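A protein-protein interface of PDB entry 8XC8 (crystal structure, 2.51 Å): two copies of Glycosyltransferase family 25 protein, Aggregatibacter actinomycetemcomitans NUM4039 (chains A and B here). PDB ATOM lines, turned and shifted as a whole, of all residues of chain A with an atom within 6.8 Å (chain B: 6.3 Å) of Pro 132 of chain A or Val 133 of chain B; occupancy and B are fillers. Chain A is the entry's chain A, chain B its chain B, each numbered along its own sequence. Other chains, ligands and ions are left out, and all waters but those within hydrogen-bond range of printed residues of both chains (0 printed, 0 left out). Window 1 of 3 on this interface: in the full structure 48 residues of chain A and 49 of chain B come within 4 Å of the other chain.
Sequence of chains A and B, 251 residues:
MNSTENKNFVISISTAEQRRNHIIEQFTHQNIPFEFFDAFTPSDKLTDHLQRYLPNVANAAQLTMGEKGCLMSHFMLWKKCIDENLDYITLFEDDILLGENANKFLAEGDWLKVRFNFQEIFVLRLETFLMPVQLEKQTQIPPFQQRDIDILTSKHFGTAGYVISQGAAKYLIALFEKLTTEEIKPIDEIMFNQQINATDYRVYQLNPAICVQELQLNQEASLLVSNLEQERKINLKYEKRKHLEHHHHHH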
ATOM      1  N   PHE A 129       2.002 -11.877  -3.721  1.00  0.00           N
ATOM      2  CA  PHE A 129       1.840 -10.786  -4.704  1.00  0.00           C
ATOM      3  C   PHE A 129       3.211 -10.498  -5.312  1.00  0.00           C
ATOM      4  O   PHE A 129       4.178 -10.228  -4.572  1.00  0.00           O
ATOM      5  CB  PHE A 129       1.204  -9.523  -4.128  1.00  0.00           C
ATOM      6  CG  PHE A 129       0.899  -8.542  -5.228  1.00  0.00           C
ATOM      7  CD1 PHE A 129      -0.144  -8.783  -6.108  1.00  0.00           C
ATOM      8  CD2 PHE A 129       1.717  -7.450  -5.460  1.00  0.00           C
ATOM      9  CE1 PHE A 129      -0.405  -7.920  -7.160  1.00  0.00           C
ATOM     10  CE2 PHE A 129       1.457  -6.591  -6.514  1.00  0.00           C
ATOM     11  CZ  PHE A 129       0.393  -6.822  -7.357  1.00  0.00           C
ATOM     12  N   LEU A 130       3.281 -10.666  -6.628  1.00  0.00           N
ATOM     13  CA  LEU A 130       4.454 -10.334  -7.467  1.00  0.00           C
ATOM     14  C   LEU A 130       4.097  -9.122  -8.330  1.00  0.00           C
ATOM     15  O   LEU A 130       2.976  -9.092  -8.888  1.00  0.00           O
ATOM     16  CB  LEU A 130       4.810 -11.575  -8.288  1.00  0.00           C
ATOM     17  CG  LEU A 130       4.947 -12.843  -7.450  1.00  0.00           C
ATOM     18  CD1 LEU A 130       5.183 -14.060  -8.328  1.00  0.00           C
ATOM     19  CD2 LEU A 130       6.063 -12.701  -6.423  1.00  0.00           C
ATOM     20  N   MET A 131       5.007  -8.152  -8.388  1.00  0.00           N
ATOM     21  CA  MET A 131       4.886  -6.910  -9.185  1.00  0.00           C
ATOM     22  C   MET A 131       4.321  -7.215 -10.567  1.00  0.00           C
ATOM     23  O   MET A 131       4.831  -8.062 -11.291  1.00  0.00           O
ATOM     24  CB  MET A 131       6.259  -6.260  -9.322  1.00  0.00           C
ATOM     25  CG  MET A 131       6.647  -5.439  -8.127  1.00  0.00           C
ATOM     26  SD  MET A 131       8.384  -4.608  -8.451  1.00  0.00           S
ATOM     27  CE  MET A 131       8.365  -3.723 -10.209  1.00  0.00           C
ATOM     28  N   PRO A 132       3.273  -6.488 -10.995  1.00  0.00           N
ATOM     29  CA  PRO A 132       2.717  -6.663 -12.329  1.00  0.00           C
ATOM     30  C   PRO A 132       3.601  -6.021 -13.403  1.00  0.00           C
ATOM     31  O   PRO A 132       3.155  -5.943 -14.511  1.00  0.00           O
ATOM     32  CB  PRO A 132       1.356  -5.963 -12.230  1.00  0.00           C
ATOM     33  CG  PRO A 132       1.608  -4.868 -11.238  1.00  0.00           C
ATOM     34  CD  PRO A 132       2.561  -5.464 -10.227  1.00  0.00           C
ATOM     35  N   VAL A 133       4.808  -5.569 -13.057  1.00  0.00           N
ATOM     36  CA  VAL A 133       5.772  -4.993 -14.037  1.00  0.00           C
ATOM     37  C   VAL A 133       7.154  -5.603 -13.786  1.00  0.00           C
ATOM     38  O   VAL A 133       7.493  -5.848 -12.610  1.00  0.00           O
ATOM     39  CB  VAL A 133       5.789  -3.456 -13.964  1.00  0.00           C
ATOM     40  CG1 VAL A 133       6.804  -2.849 -14.918  1.00  0.00           C
ATOM     41  CG2 VAL A 133       4.405  -2.880 -14.227  1.00  0.00           C
ATOM     42  N   GLN A 134       7.884  -5.897 -14.865  1.00  0.00           N
ATOM     43  CA  GLN A 134       9.298  -6.351 -14.846  1.00  0.00           C
ATOM     44  C   GLN A 134       9.885  -6.093 -16.239  1.00  0.00           C
ATOM     45  O   GLN A 134       9.118  -5.689 -17.140  1.00  0.00           O
ATOM     46  CB  GLN A 134       9.368  -7.804 -14.369  1.00  0.00           C
ATOM     47  CG  GLN A 134       8.671  -8.809 -15.275  1.00  0.00           C
ATOM     48  CD  GLN A 134       7.160  -8.731 -15.272  1.00  0.00           C
ATOM     49  OE1 GLN A 134       6.489  -8.946 -14.262  1.00  0.00           O
ATOM     50  NE2 GLN A 134       6.610  -8.433 -16.433  1.00  0.00           N
ATOM     51  N   THR A 153       7.451  -4.993 -19.315  1.00  0.00           N
ATOM     52  CA  THR A 153       6.278  -5.884 -19.515  1.00  0.00           C
ATOM     53  C   THR A 153       5.286  -5.633 -18.375  1.00  0.00           C
ATOM     54  O   THR A 153       5.726  -5.100 -17.336  1.00  0.00           O
ATOM     55  CB  THR A 153       6.713  -7.354 -19.569  1.00  0.00           C
ATOM     56  OG1 THR A 153       8.065  -7.431 -20.025  1.00  0.00           O
ATOM     57  CG2 THR A 153       5.795  -8.173 -20.446  1.00  0.00           C
ATOM     58  N   SER A 154       4.010  -5.991 -18.558  1.00  0.00           N
ATOM     59  CA  SER A 154       2.952  -5.901 -17.512  1.00  0.00           C
ATOM     60  C   SER A 154       2.286  -7.265 -17.315  1.00  0.00           C
ATOM     61  O   SER A 154       1.033  -7.317 -17.389  1.00  0.00           O
ATOM     62  CB  SER A 154       1.913  -4.832 -17.810  1.00  0.00           C
ATOM     63  OG  SER A 154       0.852  -4.853 -16.861  1.00  0.00           O
ATOM     64  N   LYS A 155       3.069  -8.315 -17.044  1.00  0.00           N
ATOM     65  CA  LYS A 155       2.543  -9.633 -16.594  1.00  0.00           C
ATOM     66  C   LYS A 155       2.182  -9.520 -15.108  1.00  0.00           C
ATOM     67  O   LYS A 155       2.926  -8.858 -14.371  1.00  0.00           O
ATOM     68  CB  LYS A 155       3.542 -10.760 -16.880  1.00  0.00           C
ATOM     69  CG  LYS A 155       3.655 -11.145 -18.348  1.00  0.00           C
ATOM     70  CD  LYS A 155       5.000 -11.715 -18.742  1.00  0.00           C
ATOM     71  CE  LYS A 155       5.210 -11.729 -20.241  1.00  0.00           C
ATOM     72  NZ  LYS A 155       6.641 -11.880 -20.594  1.00  0.00           N
ATOM     73  N   HIS A 156       1.045 -10.109 -14.722  1.00  0.00           N
ATOM     74  CA  HIS A 156       0.395  -9.993 -13.392  1.00  0.00           C
ATOM     75  C   HIS A 156       0.313 -11.423 -12.829  1.00  0.00           C
ATOM     76  O   HIS A 156      -0.793 -12.001 -12.776  1.00  0.00           O
ATOM     77  CB  HIS A 156      -0.942  -9.252 -13.587  1.00  0.00           C
ATOM     78  CG  HIS A 156      -1.344  -8.286 -12.520  1.00  0.00           C
ATOM     79  ND1 HIS A 156      -1.420  -8.631 -11.178  1.00  0.00           N
ATOM     80  CD2 HIS A 156      -1.781  -7.011 -12.608  1.00  0.00           C
ATOM     81  CE1 HIS A 156      -1.853  -7.597 -10.486  1.00  0.00           C
ATOM     82  NE2 HIS A 156      -2.080  -6.591 -11.338  1.00  0.00           N
ATOM     83  N   PHE A 157       1.475 -11.994 -12.504  1.00  0.00           N
ATOM     84  CA  PHE A 157       1.641 -13.418 -12.117  1.00  0.00           C
ATOM     85  C   PHE A 157       0.920 -13.656 -10.789  1.00  0.00           C
ATOM     86  O   PHE A 157       1.553 -13.637  -9.725  1.00  0.00           O
ATOM     87  CB  PHE A 157       3.120 -13.788 -12.034  1.00  0.00           C
ATOM     88  CG  PHE A 157       3.891 -13.519 -13.297  1.00  0.00           C
ATOM     89  CD1 PHE A 157       3.734 -14.327 -14.414  1.00  0.00           C
ATOM     90  CD2 PHE A 157       4.779 -12.458 -13.364  1.00  0.00           C
ATOM     91  CE1 PHE A 157       4.447 -14.070 -15.575  1.00  0.00           C
ATOM     92  CE2 PHE A 157       5.498 -12.210 -14.523  1.00  0.00           C
ATOM     93  CZ  PHE A 157       5.335 -13.019 -15.623  1.00  0.00           C
ATOM     94  N   ASN A 193      -6.107  -6.845 -13.011  1.00  0.00           N
ATOM     95  CA  ASN A 193      -5.726  -5.478 -13.452  1.00  0.00           C
ATOM     96  C   ASN A 193      -6.986  -4.727 -13.885  1.00  0.00           C
ATOM     97  O   ASN A 193      -7.448  -3.862 -13.114  1.00  0.00           O
ATOM     98  CB  ASN A 193      -4.675  -5.555 -14.562  1.00  0.00           C
ATOM     99  CG  ASN A 193      -4.123  -4.216 -15.002  1.00  0.00           C
ATOM    100  OD1 ASN A 193      -4.667  -3.157 -14.695  1.00  0.00           O
ATOM    101  ND2 ASN A 193      -3.019  -4.260 -15.728  1.00  0.00           N
ATOM    102  N   GLU A 220      12.135 -10.816  -9.434  1.00  0.00           N
ATOM    103  CA  GLU A 220      11.503  -9.614  -8.834  1.00  0.00           C
ATOM    104  C   GLU A 220      12.457  -9.049  -7.782  1.00  0.00           C
ATOM    105  O   GLU A 220      12.753  -7.850  -7.840  1.00  0.00           O
ATOM    106  CB  GLU A 220      10.144  -9.931  -8.212  1.00  0.00           C
ATOM    107  CG  GLU A 220       9.721  -8.918  -7.157  1.00  0.00           C
ATOM    108  CD  GLU A 220       8.318  -9.102  -6.606  1.00  0.00           C
ATOM    109  OE1 GLU A 220       8.175  -9.505  -5.420  1.00  0.00           O
ATOM    110  OE2 GLU A 220       7.366  -8.836  -7.361  1.00  0.00           O
ATOM    111  N   PHE B 129      11.954   2.714 -10.090  1.00  0.00           N
ATOM    112  CA  PHE B 129      10.579   2.235  -9.791  1.00  0.00           C
ATOM    113  C   PHE B 129      10.093   2.798  -8.453  1.00  0.00           C
ATOM    114  O   PHE B 129      10.880   2.938  -7.490  1.00  0.00           O
ATOM    115  CB  PHE B 129      10.516   0.711  -9.812  1.00  0.00           C
ATOM    116  CG  PHE B 129      10.774   0.163 -11.186  1.00  0.00           C
ATOM    117  CD1 PHE B 129       9.834   0.316 -12.189  1.00  0.00           C
ATOM    118  CD2 PHE B 129      11.978  -0.441 -11.493  1.00  0.00           C
ATOM    119  CE1 PHE B 129      10.069  -0.179 -13.462  1.00  0.00           C
ATOM    120  CE2 PHE B 129      12.213  -0.933 -12.766  1.00  0.00           C
ATOM    121  CZ  PHE B 129      11.258  -0.806 -13.748  1.00  0.00           C
ATOM    122  N   LEU B 130       8.782   3.032  -8.386  1.00  0.00           N
ATOM    123  CA  LEU B 130       8.060   3.565  -7.203  1.00  0.00           C
ATOM    124  C   LEU B 130       7.524   2.381  -6.384  1.00  0.00           C
ATOM    125  O   LEU B 130       6.905   1.472  -6.984  1.00  0.00           O
ATOM    126  CB  LEU B 130       6.944   4.480  -7.720  1.00  0.00           C
ATOM    127  CG  LEU B 130       6.491   5.610  -6.794  1.00  0.00           C
ATOM    128  CD1 LEU B 130       5.730   6.673  -7.575  1.00  0.00           C
ATOM    129  CD2 LEU B 130       5.635   5.071  -5.656  1.00  0.00           C
ATOM    130  N   MET B 131       7.828   2.362  -5.080  1.00  0.00           N
ATOM    131  CA  MET B 131       7.293   1.394  -4.079  1.00  0.00           C
ATOM    132  C   MET B 131       6.412   2.168  -3.104  1.00  0.00           C
ATOM    133  O   MET B 131       6.796   3.252  -2.674  1.00  0.00           O
ATOM    134  CB  MET B 131       8.406   0.717  -3.266  1.00  0.00           C
ATOM    135  CG  MET B 131       9.348  -0.171  -4.045  1.00  0.00           C
ATOM    136  SD  MET B 131       8.483  -1.551  -5.143  1.00  0.00           S
ATOM    137  CE  MET B 131       9.343  -1.214  -6.875  1.00  0.00           C
ATOM    138  N   PRO B 132       5.240   1.648  -2.678  1.00  0.00           N
ATOM    139  CA  PRO B 132       4.773   0.321  -3.058  1.00  0.00           C
ATOM    140  C   PRO B 132       4.149   0.360  -4.451  1.00  0.00           C
ATOM    141  O   PRO B 132       3.794   1.413  -4.874  1.00  0.00           O
ATOM    142  CB  PRO B 132       3.683  -0.029  -2.038  1.00  0.00           C
ATOM    143  CG  PRO B 132       3.549   1.183  -1.127  1.00  0.00           C
ATOM    144  CD  PRO B 132       4.285   2.324  -1.793  1.00  0.00           C
ATOM    145  N   VAL B 133       3.988  -0.792  -5.091  1.00  0.00           N
ATOM    146  CA  VAL B 133       3.320  -0.909  -6.417  1.00  0.00           C
ATOM    147  C   VAL B 133       1.814  -1.101  -6.201  1.00  0.00           C
ATOM    148  O   VAL B 133       1.053  -0.269  -6.720  1.00  0.00           O
ATOM    149  CB  VAL B 133       3.956  -2.034  -7.250  1.00  0.00           C
ATOM    150  CG1 VAL B 133       3.036  -2.544  -8.349  1.00  0.00           C
ATOM    151  CG2 VAL B 133       5.292  -1.583  -7.820  1.00  0.00           C
ATOM    152  N   GLN B 134       1.407  -2.150  -5.471  1.00  0.00           N
ATOM    153  CA  GLN B 134      -0.023  -2.465  -5.176  1.00  0.00           C
ATOM    154  C   GLN B 134      -0.379  -2.000  -3.764  1.00  0.00           C
ATOM    155  O   GLN B 134       0.396  -2.302  -2.848  1.00  0.00           O
ATOM    156  CB  GLN B 134      -0.285  -3.967  -5.269  1.00  0.00           C
ATOM    157  CG  GLN B 134      -1.757  -4.333  -5.166  1.00  0.00           C
ATOM    158  CD  GLN B 134      -2.476  -4.193  -6.485  1.00  0.00           C
ATOM    159  OE1 GLN B 134      -2.228  -4.945  -7.433  1.00  0.00           O
ATOM    160  NE2 GLN B 134      -3.406  -3.249  -6.546  1.00  0.00           N
ATOM    161  N   LEU B 135      -1.542  -1.366  -3.585  1.00  0.00           N
ATOM    162  CA  LEU B 135      -2.082  -1.048  -2.238  1.00  0.00           C
ATOM    163  C   LEU B 135      -3.123  -2.098  -1.832  1.00  0.00           C
ATOM    164  O   LEU B 135      -3.906  -2.550  -2.702  1.00  0.00           O
ATOM    165  CB  LEU B 135      -2.678   0.360  -2.237  1.00  0.00           C
ATOM    166  CG  LEU B 135      -1.669   1.502  -2.120  1.00  0.00           C
ATOM    167  CD1 LEU B 135      -2.330   2.836  -2.439  1.00  0.00           C
ATOM    168  CD2 LEU B 135      -1.031   1.534  -0.739  1.00  0.00           C
ATOM    169  N   SER B 154      -5.349  -0.201  -5.488  1.00  0.00           N
ATOM    170  CA  SER B 154      -4.849   0.582  -6.644  1.00  0.00           C
ATOM    171  C   SER B 154      -3.332   0.427  -6.770  1.00  0.00           C
ATOM    172  O   SER B 154      -2.644   0.478  -5.741  1.00  0.00           O
ATOM    173  CB  SER B 154      -5.213   2.024  -6.488  1.00  0.00           C
ATOM    174  OG  SER B 154      -4.594   2.572  -5.329  1.00  0.00           O
ATOM    175  N   LYS B 155      -2.852   0.222  -7.995  1.00  0.00           N
ATOM    176  CA  LYS B 155      -1.409   0.169  -8.333  1.00  0.00           C
ATOM    177  C   LYS B 155      -0.886   1.608  -8.454  1.00  0.00           C
ATOM    178  O   LYS B 155      -1.658   2.476  -8.880  1.00  0.00           O
ATOM    179  CB  LYS B 155      -1.221  -0.668  -9.603  1.00  0.00           C
ATOM    180  CG  LYS B 155      -1.504  -2.157  -9.433  1.00  0.00           C
ATOM    181  CD  LYS B 155      -1.912  -2.869 -10.707  1.00  0.00           C
ATOM    182  CE  LYS B 155      -3.391  -2.755 -11.023  1.00  0.00           C
ATOM    183  NZ  LYS B 155      -4.224  -3.623 -10.156  1.00  0.00           N
ATOM    184  N   HIS B 156       0.375   1.843  -8.078  1.00  0.00           N
ATOM    185  CA  HIS B 156       1.095   3.139  -8.214  1.00  0.00           C
ATOM    186  C   HIS B 156       2.426   2.964  -8.949  1.00  0.00           C
ATOM    187  O   HIS B 156       3.252   2.182  -8.480  1.00  0.00           O
ATOM    188  CB  HIS B 156       1.368   3.762  -6.843  1.00  0.00           C
ATOM    189  CG  HIS B 156       0.155   4.363  -6.221  1.00  0.00           C
ATOM    190  ND1 HIS B 156       0.036   4.532  -4.856  1.00  0.00           N
ATOM    191  CD2 HIS B 156      -0.994   4.821  -6.764  1.00  0.00           C
ATOM    192  CE1 HIS B 156      -1.132   5.079  -4.585  1.00  0.00           C
ATOM    193  NE2 HIS B 156      -1.782   5.263  -5.738  1.00  0.00           N
ATOM    194  N   PHE B 157       2.653   3.752 -10.008  1.00  0.00           N
ATOM    195  CA  PHE B 157       3.946   3.864 -10.743  1.00  0.00           C
ATOM    196  C   PHE B 157       4.362   5.340 -10.825  1.00  0.00           C
ATOM    197  O   PHE B 157       3.496   6.242 -10.767  1.00  0.00           O
ATOM    198  CB  PHE B 157       3.853   3.212 -12.127  1.00  0.00           C
ATOM    199  CG  PHE B 157       3.063   1.928 -12.137  1.00  0.00           C
ATOM    200  CD1 PHE B 157       1.679   1.960 -12.117  1.00  0.00           C
ATOM    201  CD2 PHE B 157       3.698   0.694 -12.108  1.00  0.00           C
ATOM    202  CE1 PHE B 157       0.944   0.789 -12.100  1.00  0.00           C
ATOM    203  CE2 PHE B 157       2.963  -0.478 -12.087  1.00  0.00           C
ATOM    204  CZ  PHE B 157       1.587  -0.429 -12.083  1.00  0.00           C
ATOM    205  N   ASN B 193       1.299   0.467 -16.800  1.00  0.00           N
ATOM    206  CA  ASN B 193       0.611  -0.794 -16.411  1.00  0.00           C
ATOM    207  C   ASN B 193      -0.317  -1.237 -17.549  1.00  0.00           C
ATOM    208  O   ASN B 193       0.053  -2.161 -18.301  1.00  0.00           O
ATOM    209  CB  ASN B 193      -0.149  -0.630 -15.089  1.00  0.00           C
ATOM    210  CG  ASN B 193      -0.746  -1.923 -14.570  1.00  0.00           C
ATOM    211  OD1 ASN B 193      -0.144  -2.985 -14.714  1.00  0.00           O
ATOM    212  ND2 ASN B 193      -1.932  -1.849 -13.981  1.00  0.00           N
ATOM    213  N   ILE B 196       1.060  -1.236 -21.702  1.00  0.00           N
ATOM    214  CA  ILE B 196       2.258  -1.997 -22.178  1.00  0.00           C
ATOM    215  C   ILE B 196       1.748  -3.337 -22.719  1.00  0.00           C
ATOM    216  O   ILE B 196       2.441  -3.923 -23.565  1.00  0.00           O
ATOM    217  CB  ILE B 196       3.354  -2.171 -21.104  1.00  0.00           C
ATOM    218  CG1 ILE B 196       4.610  -2.873 -21.633  1.00  0.00           C
ATOM    219  CG2 ILE B 196       2.820  -2.924 -19.907  1.00  0.00           C
ATOM    220  CD1 ILE B 196       5.218  -2.285 -22.891  1.00  0.00           C
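The side-chain amide oxygen (OD1) of Asn 193 of chain B is in hydrogen-bond range of the side-chain hydroxyl (OG) of Ser 154 of chain A (3.0 Å). The side-chain amide nitrogen (ND2) of Asn 193 of chain B sits at hydrogen-bond distance from the side-chain amide oxygen (OD1) of Asn 193 of chain A (3.1 Å).
Among the printed residues, pairs that only touch across the chains: Ser 154 of chain A with Ile 196 of chain B, Phe 129 of chain A with Gln 134 of chain B, Pro 132 of chain A with Val 133 of chain B, Val 133 of chain A with Phe 157 of chain B, His 156 of chain A with Lys 155 of chain B, Met 131 of chain A with Met 131 of chain B, Asn 193 of chain A with Lys 155 of chain B and Thr 153 of chain A with Ile 196 of chain B.
O of Pro 132 of chain A lies close to OG of Ser 154 of chain A (3.5 Å). The backbone carbonyl oxygen (O) of Pro 132 of chain A is in hydrogen-bond range of the backbone NH (N) of Lys 155 of chain A. The backbone carbonyl oxygen (O) of Val 133 of chain B sits at hydrogen-bond distance from the backbone NH (N) of His 156 of chain B (2.6 Å). The backbone carbonyl oxygen (O) of Gln 134 of chain A lies within hydrogen-bond range of the backbone NH (N) of Thr 153 of chain A (2.8 Å). The side-chain carboxylate of Glu 220 of chain A is in hydrogen-bond range of the backbone NH of Met 131 of chain A.
Phe 129 of chain A touches Gln 134 of chain B, but with the chains exchanged Gln 134 of chain A does not touch Phe 129 of chain B (6.0 Å). Pro 132 of chain A touches Val 133 of chain B, but with the chains exchanged Val 133 of chain A does not touch Pro 132 of chain B (10.3 Å). Asn 193 of chain A touches Lys 155 of chain B, but with the chains exchanged Lys 155 of chain A does not touch Asn 193 of chain B (6.6 Å). Asn 193 of chain B touches its own counterpart, Asn 193 of chain A.
Hydrophobic or aromatic side chains of chain A within 4 Å of the printed part of chain B: Phe 129, Met 131, Pro 132, Val 133 and His 156. Among the printed residues, 10 pairs touch across the chains.
Of the printed residues of chain B, Met 131 of chain A touches Met 131. Pro 132 of chain A touches just one residue of chain B: Val 133. Of the printed residues of chain B, Ser 154 of chain A touches Asn 193 and Ile 196. Of the printed residues of chain A, Lys 155 of chain B touches His 156 (3.8 Å) and Asn 193 (3.9 Å). The nearest residue of chain A that does not touch Val 133 of chain B is Met 131 of chain A (4.1 Å). The nearest printed residue of chain B that does not touch His 156 of chain A is Gln 134 of chain B (4.1 Å).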
